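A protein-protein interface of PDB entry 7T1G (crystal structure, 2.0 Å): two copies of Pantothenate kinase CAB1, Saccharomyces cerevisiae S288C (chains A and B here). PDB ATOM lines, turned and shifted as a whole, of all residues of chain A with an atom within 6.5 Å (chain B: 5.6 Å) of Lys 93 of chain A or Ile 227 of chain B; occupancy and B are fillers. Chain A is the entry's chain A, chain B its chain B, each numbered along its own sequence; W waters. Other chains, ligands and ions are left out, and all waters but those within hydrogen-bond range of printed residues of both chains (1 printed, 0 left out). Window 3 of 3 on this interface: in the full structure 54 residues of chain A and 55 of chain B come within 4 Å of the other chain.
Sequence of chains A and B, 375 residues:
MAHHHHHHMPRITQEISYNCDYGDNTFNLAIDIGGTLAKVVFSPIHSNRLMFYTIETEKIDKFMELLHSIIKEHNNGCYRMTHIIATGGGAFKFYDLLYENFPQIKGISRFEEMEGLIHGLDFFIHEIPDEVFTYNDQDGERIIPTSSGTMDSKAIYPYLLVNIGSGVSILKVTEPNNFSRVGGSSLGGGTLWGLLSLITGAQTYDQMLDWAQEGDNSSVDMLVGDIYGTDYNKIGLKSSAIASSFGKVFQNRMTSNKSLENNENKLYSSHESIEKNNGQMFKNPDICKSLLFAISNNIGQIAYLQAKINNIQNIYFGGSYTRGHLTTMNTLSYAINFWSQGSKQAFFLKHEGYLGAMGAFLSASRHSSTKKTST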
ATOM      1  N   ILE A  33      11.016  12.970 -28.317  1.00  0.00           N
ATOM      2  CA  ILE A  33      12.402  12.554 -28.444  1.00  0.00           C
ATOM      3  C   ILE A  33      12.511  11.734 -29.722  1.00  0.00           C
ATOM      4  O   ILE A  33      11.833  10.713 -29.850  1.00  0.00           O
ATOM      5  CB  ILE A  33      12.844  11.732 -27.223  1.00  0.00           C
ATOM      6  CG1 ILE A  33      12.518  12.458 -25.913  1.00  0.00           C
ATOM      7  CG2 ILE A  33      14.319  11.373 -27.346  1.00  0.00           C
ATOM      8  CD1 ILE A  33      12.750  11.581 -24.675  1.00  0.00           C
ATOM      9  N   GLY A  34      13.324  12.209 -30.664  1.00  0.00           N
ATOM     10  CA  GLY A  34      13.500  11.481 -31.909  1.00  0.00           C
ATOM     11  C   GLY A  34      14.888  10.842 -31.979  1.00  0.00           C
ATOM     12  O   GLY A  34      15.571  10.705 -30.962  1.00  0.00           O
ATOM     13  N   GLY A  35      15.270  10.408 -33.189  1.00  0.00           N
ATOM     14  CA  GLY A  35      16.602   9.894 -33.439  1.00  0.00           C
ATOM     15  C   GLY A  35      17.682  10.899 -33.045  1.00  0.00           C
ATOM     16  O   GLY A  35      18.673  10.492 -32.455  1.00  0.00           O
ATOM     17  N   THR A  36      17.464  12.195 -33.349  1.00  0.00           N
ATOM     18  CA  THR A  36      18.486  13.225 -33.246  1.00  0.00           C
ATOM     19  C   THR A  36      18.109  14.319 -32.251  1.00  0.00           C
ATOM     20  O   THR A  36      18.988  14.770 -31.518  1.00  0.00           O
ATOM     21  CB  THR A  36      18.763  13.909 -34.592  1.00  0.00           C
ATOM     22  OG1 THR A  36      19.006  12.894 -35.573  1.00  0.00           O
ATOM     23  CG2 THR A  36      19.940  14.857 -34.542  1.00  0.00           C
ATOM     24  N   GLY A  88       7.431  10.583 -29.416  1.00  0.00           N
ATOM     25  CA  GLY A  88       8.464  10.363 -30.406  1.00  0.00           C
ATOM     26  C   GLY A  88       8.996   8.947 -30.241  1.00  0.00           C
ATOM     27  O   GLY A  88       8.684   8.297 -29.252  1.00  0.00           O
ATOM     28  N   GLY A  89       9.804   8.478 -31.197  1.00  0.00           N
ATOM     29  CA  GLY A  89      10.372   7.140 -31.131  1.00  0.00           C
ATOM     30  C   GLY A  89      11.225   6.898 -29.884  1.00  0.00           C
ATOM     31  O   GLY A  89      11.343   5.757 -29.430  1.00  0.00           O
ATOM     32  N   GLY A  90      11.821   7.964 -29.331  1.00  0.00           N
ATOM     33  CA  GLY A  90      12.768   7.843 -28.224  1.00  0.00           C
ATOM     34  C   GLY A  90      12.112   7.858 -26.844  1.00  0.00           C
ATOM     35  O   GLY A  90      12.822   7.792 -25.834  1.00  0.00           O
ATOM     36  N   ALA A  91      10.764   7.942 -26.808  1.00  0.00           N
ATOM     37  CA  ALA A  91      10.008   7.890 -25.561  1.00  0.00           C
ATOM     38  C   ALA A  91      10.297   6.586 -24.817  1.00  0.00           C
ATOM     39  O   ALA A  91      10.291   6.553 -23.591  1.00  0.00           O
ATOM     40  CB  ALA A  91       8.521   8.010 -25.829  1.00  0.00           C
ATOM     41  N   PHE A  92      10.480   5.500 -25.580  1.00  0.00           N
ATOM     42  CA  PHE A  92      10.719   4.168 -25.047  1.00  0.00           C
ATOM     43  C   PHE A  92      12.155   4.084 -24.550  1.00  0.00           C
ATOM     44  O   PHE A  92      12.380   3.748 -23.398  1.00  0.00           O
ATOM     45  CB  PHE A  92      10.422   3.102 -26.107  1.00  0.00           C
ATOM     46  CG  PHE A  92       9.004   3.119 -26.629  1.00  0.00           C
ATOM     47  CD1 PHE A  92       7.958   2.576 -25.886  1.00  0.00           C
ATOM     48  CD2 PHE A  92       8.708   3.685 -27.867  1.00  0.00           C
ATOM     49  CE1 PHE A  92       6.653   2.596 -26.364  1.00  0.00           C
ATOM     50  CE2 PHE A  92       7.404   3.708 -28.347  1.00  0.00           C
ATOM     51  CZ  PHE A  92       6.378   3.162 -27.596  1.00  0.00           C
ATOM     52  N   LYS A  93      13.098   4.464 -25.419  1.00  0.00           N
ATOM     53  CA  LYS A  93      14.521   4.292 -25.176  1.00  0.00           C
ATOM     54  C   LYS A  93      14.977   5.107 -23.971  1.00  0.00           C
ATOM     55  O   LYS A  93      15.908   4.697 -23.301  1.00  0.00           O
ATOM     56  CB  LYS A  93      15.321   4.727 -26.409  1.00  0.00           C
ATOM     57  CG  LYS A  93      16.831   4.854 -26.214  1.00  0.00           C
ATOM     58  CD  LYS A  93      17.594   5.204 -27.478  1.00  0.00           C
ATOM     59  CE  LYS A  93      19.082   5.354 -27.257  1.00  0.00           C
ATOM     60  NZ  LYS A  93      19.806   5.405 -28.553  1.00  0.00           N
ATOM     61  N   PHE A  94      14.362   6.282 -23.742  1.00  0.00           N
ATOM     62  CA  PHE A  94      14.833   7.259 -22.760  1.00  0.00           C
ATOM     63  C   PHE A  94      13.989   7.233 -21.482  1.00  0.00           C
ATOM     64  O   PHE A  94      14.194   8.035 -20.575  1.00  0.00           O
ATOM     65  CB  PHE A  94      14.806   8.672 -23.361  1.00  0.00           C
ATOM     66  CG  PHE A  94      15.942   8.934 -24.319  1.00  0.00           C
ATOM     67  CD1 PHE A  94      17.044   9.676 -23.925  1.00  0.00           C
ATOM     68  CD2 PHE A  94      15.917   8.434 -25.614  1.00  0.00           C
ATOM     69  CE1 PHE A  94      18.090   9.922 -24.809  1.00  0.00           C
ATOM     70  CE2 PHE A  94      16.969   8.665 -26.493  1.00  0.00           C
ATOM     71  CZ  PHE A  94      18.063   9.394 -26.084  1.00  0.00           C
ATOM     72  N   TYR A  95      13.055   6.297 -21.412  1.00  0.00           N
ATOM     73  CA  TYR A  95      12.147   6.262 -20.286  1.00  0.00           C
ATOM     74  C   TYR A  95      12.932   6.084 -18.979  1.00  0.00           C
ATOM     75  O   TYR A  95      12.655   6.758 -17.981  1.00  0.00           O
ATOM     76  CB  TYR A  95      11.049   5.216 -20.531  1.00  0.00           C
ATOM     77  CG  TYR A  95      10.044   5.212 -19.413  1.00  0.00           C
ATOM     78  CD1 TYR A  95       8.851   5.916 -19.514  1.00  0.00           C
ATOM     79  CD2 TYR A  95      10.350   4.598 -18.205  1.00  0.00           C
ATOM     80  CE1 TYR A  95       7.954   5.949 -18.455  1.00  0.00           C
ATOM     81  CE2 TYR A  95       9.470   4.640 -17.131  1.00  0.00           C
ATOM     82  CZ  TYR A  95       8.269   5.314 -17.258  1.00  0.00           C
ATOM     83  OH  TYR A  95       7.426   5.333 -16.182  1.00  0.00           O
ATOM     84  N   ASP A  96      13.936   5.193 -18.988  1.00  0.00           N
ATOM     85  CA  ASP A  96      14.703   4.935 -17.778  1.00  0.00           C
ATOM     86  C   ASP A  96      15.608   6.110 -17.414  1.00  0.00           C
ATOM     87  O   ASP A  96      15.815   6.374 -16.224  1.00  0.00           O
ATOM     88  CB  ASP A  96      15.531   3.662 -17.892  1.00  0.00           C
ATOM     89  CG  ASP A  96      14.659   2.438 -17.722  1.00  0.00           C
ATOM     90  OD1 ASP A  96      13.693   2.505 -16.930  1.00  0.00           O
ATOM     91  OD2 ASP A  96      14.922   1.452 -18.413  1.00  0.00           O
ATOM     92  N   LEU A  97      16.165   6.790 -18.427  1.00  0.00           N
ATOM     93  CA  LEU A  97      16.979   7.965 -18.158  1.00  0.00           C
ATOM     94  C   LEU A  97      16.123   9.025 -17.460  1.00  0.00           C
ATOM     95  O   LEU A  97      16.572   9.672 -16.507  1.00  0.00           O
ATOM     96  CB  LEU A  97      17.565   8.514 -19.465  1.00  0.00           C
ATOM     97  CG  LEU A  97      19.036   8.168 -19.714  1.00  0.00           C
ATOM     98  CD1 LEU A  97      19.382   8.332 -21.190  1.00  0.00           C
ATOM     99  CD2 LEU A  97      19.970   9.018 -18.841  1.00  0.00           C
ATOM    100  N   GLU A 113       3.254   8.098 -30.874  1.00  0.00           N
ATOM    101  CA  GLU A 113       3.922   9.059 -31.728  1.00  0.00           C
ATOM    102  C   GLU A 113       2.966   9.654 -32.759  1.00  0.00           C
ATOM    103  O   GLU A 113       2.970  10.867 -32.999  1.00  0.00           O
ATOM    104  CB  GLU A 113       5.088   8.323 -32.391  1.00  0.00           C
ATOM    105  CG  GLU A 113       5.631   9.010 -33.625  1.00  0.00           C
ATOM    106  CD  GLU A 113       6.866   8.333 -34.193  1.00  0.00           C
ATOM    107  OE1 GLU A 113       7.166   7.194 -33.779  1.00  0.00           O
ATOM    108  OE2 GLU A 113       7.514   8.948 -35.053  1.00  0.00           O
ATOM    109  N   SER A 166      14.967  12.288 -38.503  1.00  0.00           N
ATOM    110  CA  SER A 166      16.027  11.408 -38.985  1.00  0.00           C
ATOM    111  C   SER A 166      15.608  10.724 -40.294  1.00  0.00           C
ATOM    112  O   SER A 166      16.337  10.771 -41.283  1.00  0.00           O
ATOM    113  CB  SER A 166      16.373  10.387 -37.937  1.00  0.00           C
ATOM    114  OG  SER A 166      16.582  11.059 -36.706  1.00  0.00           O
ATOM    115  N   GLY A 167      14.480   9.994 -40.233  1.00  0.00           N
ATOM    116  CA  GLY A 167      13.815   9.449 -41.414  1.00  0.00           C
ATOM    117  C   GLY A 167      12.624  10.337 -41.799  1.00  0.00           C
ATOM    118  O   GLY A 167      12.551  11.496 -41.395  1.00  0.00           O
ATOM    119  N   MET B 222      20.711   4.606 -38.718  1.00  0.00           N
ATOM    120  CA  MET B 222      19.805   4.386 -37.598  1.00  0.00           C
ATOM    121  C   MET B 222      18.756   3.364 -37.994  1.00  0.00           C
ATOM    122  O   MET B 222      17.981   3.621 -38.903  1.00  0.00           O
ATOM    123  CB  MET B 222      19.037   5.644 -37.190  1.00  0.00           C
ATOM    124  CG  MET B 222      19.776   6.496 -36.204  1.00  0.00           C
ATOM    125  SD  MET B 222      18.806   8.026 -36.085  1.00  0.00           S
ATOM    126  CE  MET B 222      20.070   9.156 -35.504  1.00  0.00           C
ATOM    127  N   LEU B 223      18.708   2.245 -37.267  1.00  0.00           N
ATOM    128  CA  LEU B 223      17.668   1.254 -37.468  1.00  0.00           C
ATOM    129  C   LEU B 223      16.516   1.552 -36.500  1.00  0.00           C
ATOM    130  O   LEU B 223      16.626   2.401 -35.617  1.00  0.00           O
ATOM    131  CB  LEU B 223      18.263  -0.138 -37.213  1.00  0.00           C
ATOM    132  CG  LEU B 223      19.588  -0.414 -37.940  1.00  0.00           C
ATOM    133  CD1 LEU B 223      20.085  -1.838 -37.685  1.00  0.00           C
ATOM    134  CD2 LEU B 223      19.465  -0.140 -39.434  1.00  0.00           C
ATOM    135  N   VAL B 224      15.385   0.888 -36.711  1.00  0.00           N
ATOM    136  CA  VAL B 224      14.232   1.094 -35.848  1.00  0.00           C
ATOM    137  C   VAL B 224      14.681   0.898 -34.400  1.00  0.00           C
ATOM    138  O   VAL B 224      14.459   1.759 -33.538  1.00  0.00           O
ATOM    139  CB  VAL B 224      13.100   0.111 -36.218  1.00  0.00           C
ATOM    140  CG1 VAL B 224      11.917   0.216 -35.260  1.00  0.00           C
ATOM    141  CG2 VAL B 224      12.659   0.291 -37.649  1.00  0.00           C
ATOM    142  N   GLY B 225      15.352  -0.234 -34.156  1.00  0.00           N
ATOM    143  CA  GLY B 225      15.843  -0.601 -32.836  1.00  0.00           C
ATOM    144  C   GLY B 225      16.659   0.503 -32.165  1.00  0.00           C
ATOM    145  O   GLY B 225      16.634   0.621 -30.941  1.00  0.00           O
ATOM    146  N   ASP B 226      17.396   1.284 -32.971  1.00  0.00           N
ATOM    147  CA  ASP B 226      18.241   2.369 -32.504  1.00  0.00           C
ATOM    148  C   ASP B 226      17.371   3.522 -31.999  1.00  0.00           C
ATOM    149  O   ASP B 226      17.738   4.231 -31.061  1.00  0.00           O
ATOM    150  CB  ASP B 226      19.211   2.848 -33.598  1.00  0.00           C
ATOM    151  CG  ASP B 226      20.217   1.778 -34.012  1.00  0.00           C
ATOM    152  OD1 ASP B 226      20.578   0.936 -33.159  1.00  0.00           O
ATOM    153  OD2 ASP B 226      20.617   1.762 -35.191  1.00  0.00           O
ATOM    154  N   ILE B 227      16.223   3.718 -32.642  1.00  0.00           N
ATOM    155  CA  ILE B 227      15.334   4.805 -32.272  1.00  0.00           C
ATOM    156  C   ILE B 227      14.474   4.406 -31.061  1.00  0.00           C
ATOM    157  O   ILE B 227      14.277   5.223 -30.153  1.00  0.00           O
ATOM    158  CB  ILE B 227      14.543   5.284 -33.507  1.00  0.00           C
ATOM    159  CG1 ILE B 227      15.494   5.942 -34.519  1.00  0.00           C
ATOM    160  CG2 ILE B 227      13.428   6.231 -33.104  1.00  0.00           C
ATOM    161  CD1 ILE B 227      14.847   6.921 -35.486  1.00  0.00           C
ATOM    162  N   TYR B 228      14.001   3.145 -31.052  1.00  0.00           N
ATOM    163  CA  TYR B 228      13.261   2.534 -29.947  1.00  0.00           C
ATOM    164  C   TYR B 228      14.190   1.616 -29.124  1.00  0.00           C
ATOM    165  O   TYR B 228      14.198   0.368 -29.351  1.00  0.00           O
ATOM    166  CB  TYR B 228      12.017   1.809 -30.480  1.00  0.00           C
ATOM    167  CG  TYR B 228      11.200   2.623 -31.459  1.00  0.00           C
ATOM    168  CD1 TYR B 228      11.696   2.982 -32.702  1.00  0.00           C
ATOM    169  CD2 TYR B 228       9.926   3.059 -31.138  1.00  0.00           C
ATOM    170  CE1 TYR B 228      10.960   3.750 -33.595  1.00  0.00           C
ATOM    171  CE2 TYR B 228       9.176   3.829 -32.018  1.00  0.00           C
ATOM    172  CZ  TYR B 228       9.696   4.190 -33.247  1.00  0.00           C
ATOM    173  OH  TYR B 228       8.961   4.960 -34.111  1.00  0.00           O
ATOM    174  N   ALA B 243      15.538   3.107 -40.248  1.00  0.00           N
ATOM    175  CA  ALA B 243      14.765   4.321 -40.000  1.00  0.00           C
ATOM    176  C   ALA B 243      15.402   5.539 -40.678  1.00  0.00           C
ATOM    177  O   ALA B 243      14.711   6.403 -41.205  1.00  0.00           O
ATOM    178  CB  ALA B 243      14.646   4.544 -38.495  1.00  0.00           C
HETATM  179  O   HOH W   1      15.959   7.880 -30.027  1.00  0.00           O
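The side-chain hydroxyl of Ser 166 of chain A lies within hydrogen-bond range of the side-chain hydroxyl of Thr 36 of chain A.
The backbone NH (N) of Leu 223 of chain B lies within hydrogen-bond range of the side-chain carboxylate (OD2) of Asp 226 of chain B, at 2.9 Å.
The backbone NH (N) of Gly 89 of chain A is in hydrogen-bond range of the backbone carbonyl oxygen (O) of Ile 33 of chain A (3.3 Å).
The backbone carbonyl oxygen (O) of Met 222 of chain B lies within hydrogen-bond range of the backbone NH (N) of Ala 243 of chain B.
The backbone carbonyl oxygen of Ile 33 of chain A is in hydrogen-bond range of the backbone NH of Gly 90 of chain A, 2.8 Å away.
Of chain B, only Asp 226 and Ile 227 come within 4 Å of Lys 93 of chain A.
Of the printed residues of chain B, Gly 90 of chain A touches Ile 227 (3.6 Å).
Printed residues of chain B within 4 Å of Thr 36 of chain A: Met 222.
Printed residues of chain B within 4 Å of Gly 89 of chain A: Ile 227 and Tyr 228.
Printed residues of chain B within 4 Å of Gly 35 of chain A: Met 222 (3.6 Å).
Printed residues of chain A within 4 Å of Met 222 of chain B: Gly 35, Thr 36 and Ser 166.
Tyr 95 of chain A touches none of the printed residues of chain B.
Asp 96 of chain A touches none of the printed residues of chain B.
The nearest printed residue of chain B that does not touch Gly 35 of chain A is Ile 227 of chain B (4.01 Å).
Water W1 bridges O of Gly 34 of chain A (3.0 Å) and O of Ile 227 of chain B (3.1 Å).
Printed residues of chain A that touch a printed residue of chain B: Gly 35, Thr 36, Gly 89, Gly 90, Phe 92, Lys 93, Glu 113, Ser 166 and Gly 167.
Hydrophobic or aromatic side chains of chain A that line the printed part of chain B: Phe 92.
Hydrophobic or aromatic side chains of chain B within 4 Å of the printed part of chain A: Met 222, Ile 227 and Tyr 228.
Among the printed residues, 11 pairs touch across the chains.
O of Asp 226 of chain B lies within hydrogen-bond range of NZ of Lys 93 of chain A (3.5 Å).
O of Gly 89 of chain A sits close to O of Ile 227 of chain B, at 3.1 Å.
OE1 of Glu 113 of chain A sits at hydrogen-bond distance from OH of Tyr 228 of chain B.
Gly 35 of chain A touches Met 222 of chain B (O to CE, 3.6 Å).
CE of Met 222 of chain B touches OG1 of Thr 36 of chain A, 3.9 Å away.
Tyr 228 of chain B touches Gly 89 of chain A.
Ile 227 of chain B touches Gly 90 of chain A (O to CA, 3.6 Å).
Phe 92 of chain A touches Tyr 228 of chain B.
Ile 227 of chain B touches Lys 93 of chain A (O to CB, 3.9 Å).
OG of Ser 166 of chain A touches SD of Met 222 of chain B, 3.8 Å away.
O of Ala 243 of chain B touches CA of Gly 167 of chain A, at 3.2 Å.
No position is printed for both chains.
Of the 11 pairs that touch across the chains among the printed residues, none has its exchanged pair printed and touching as well.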
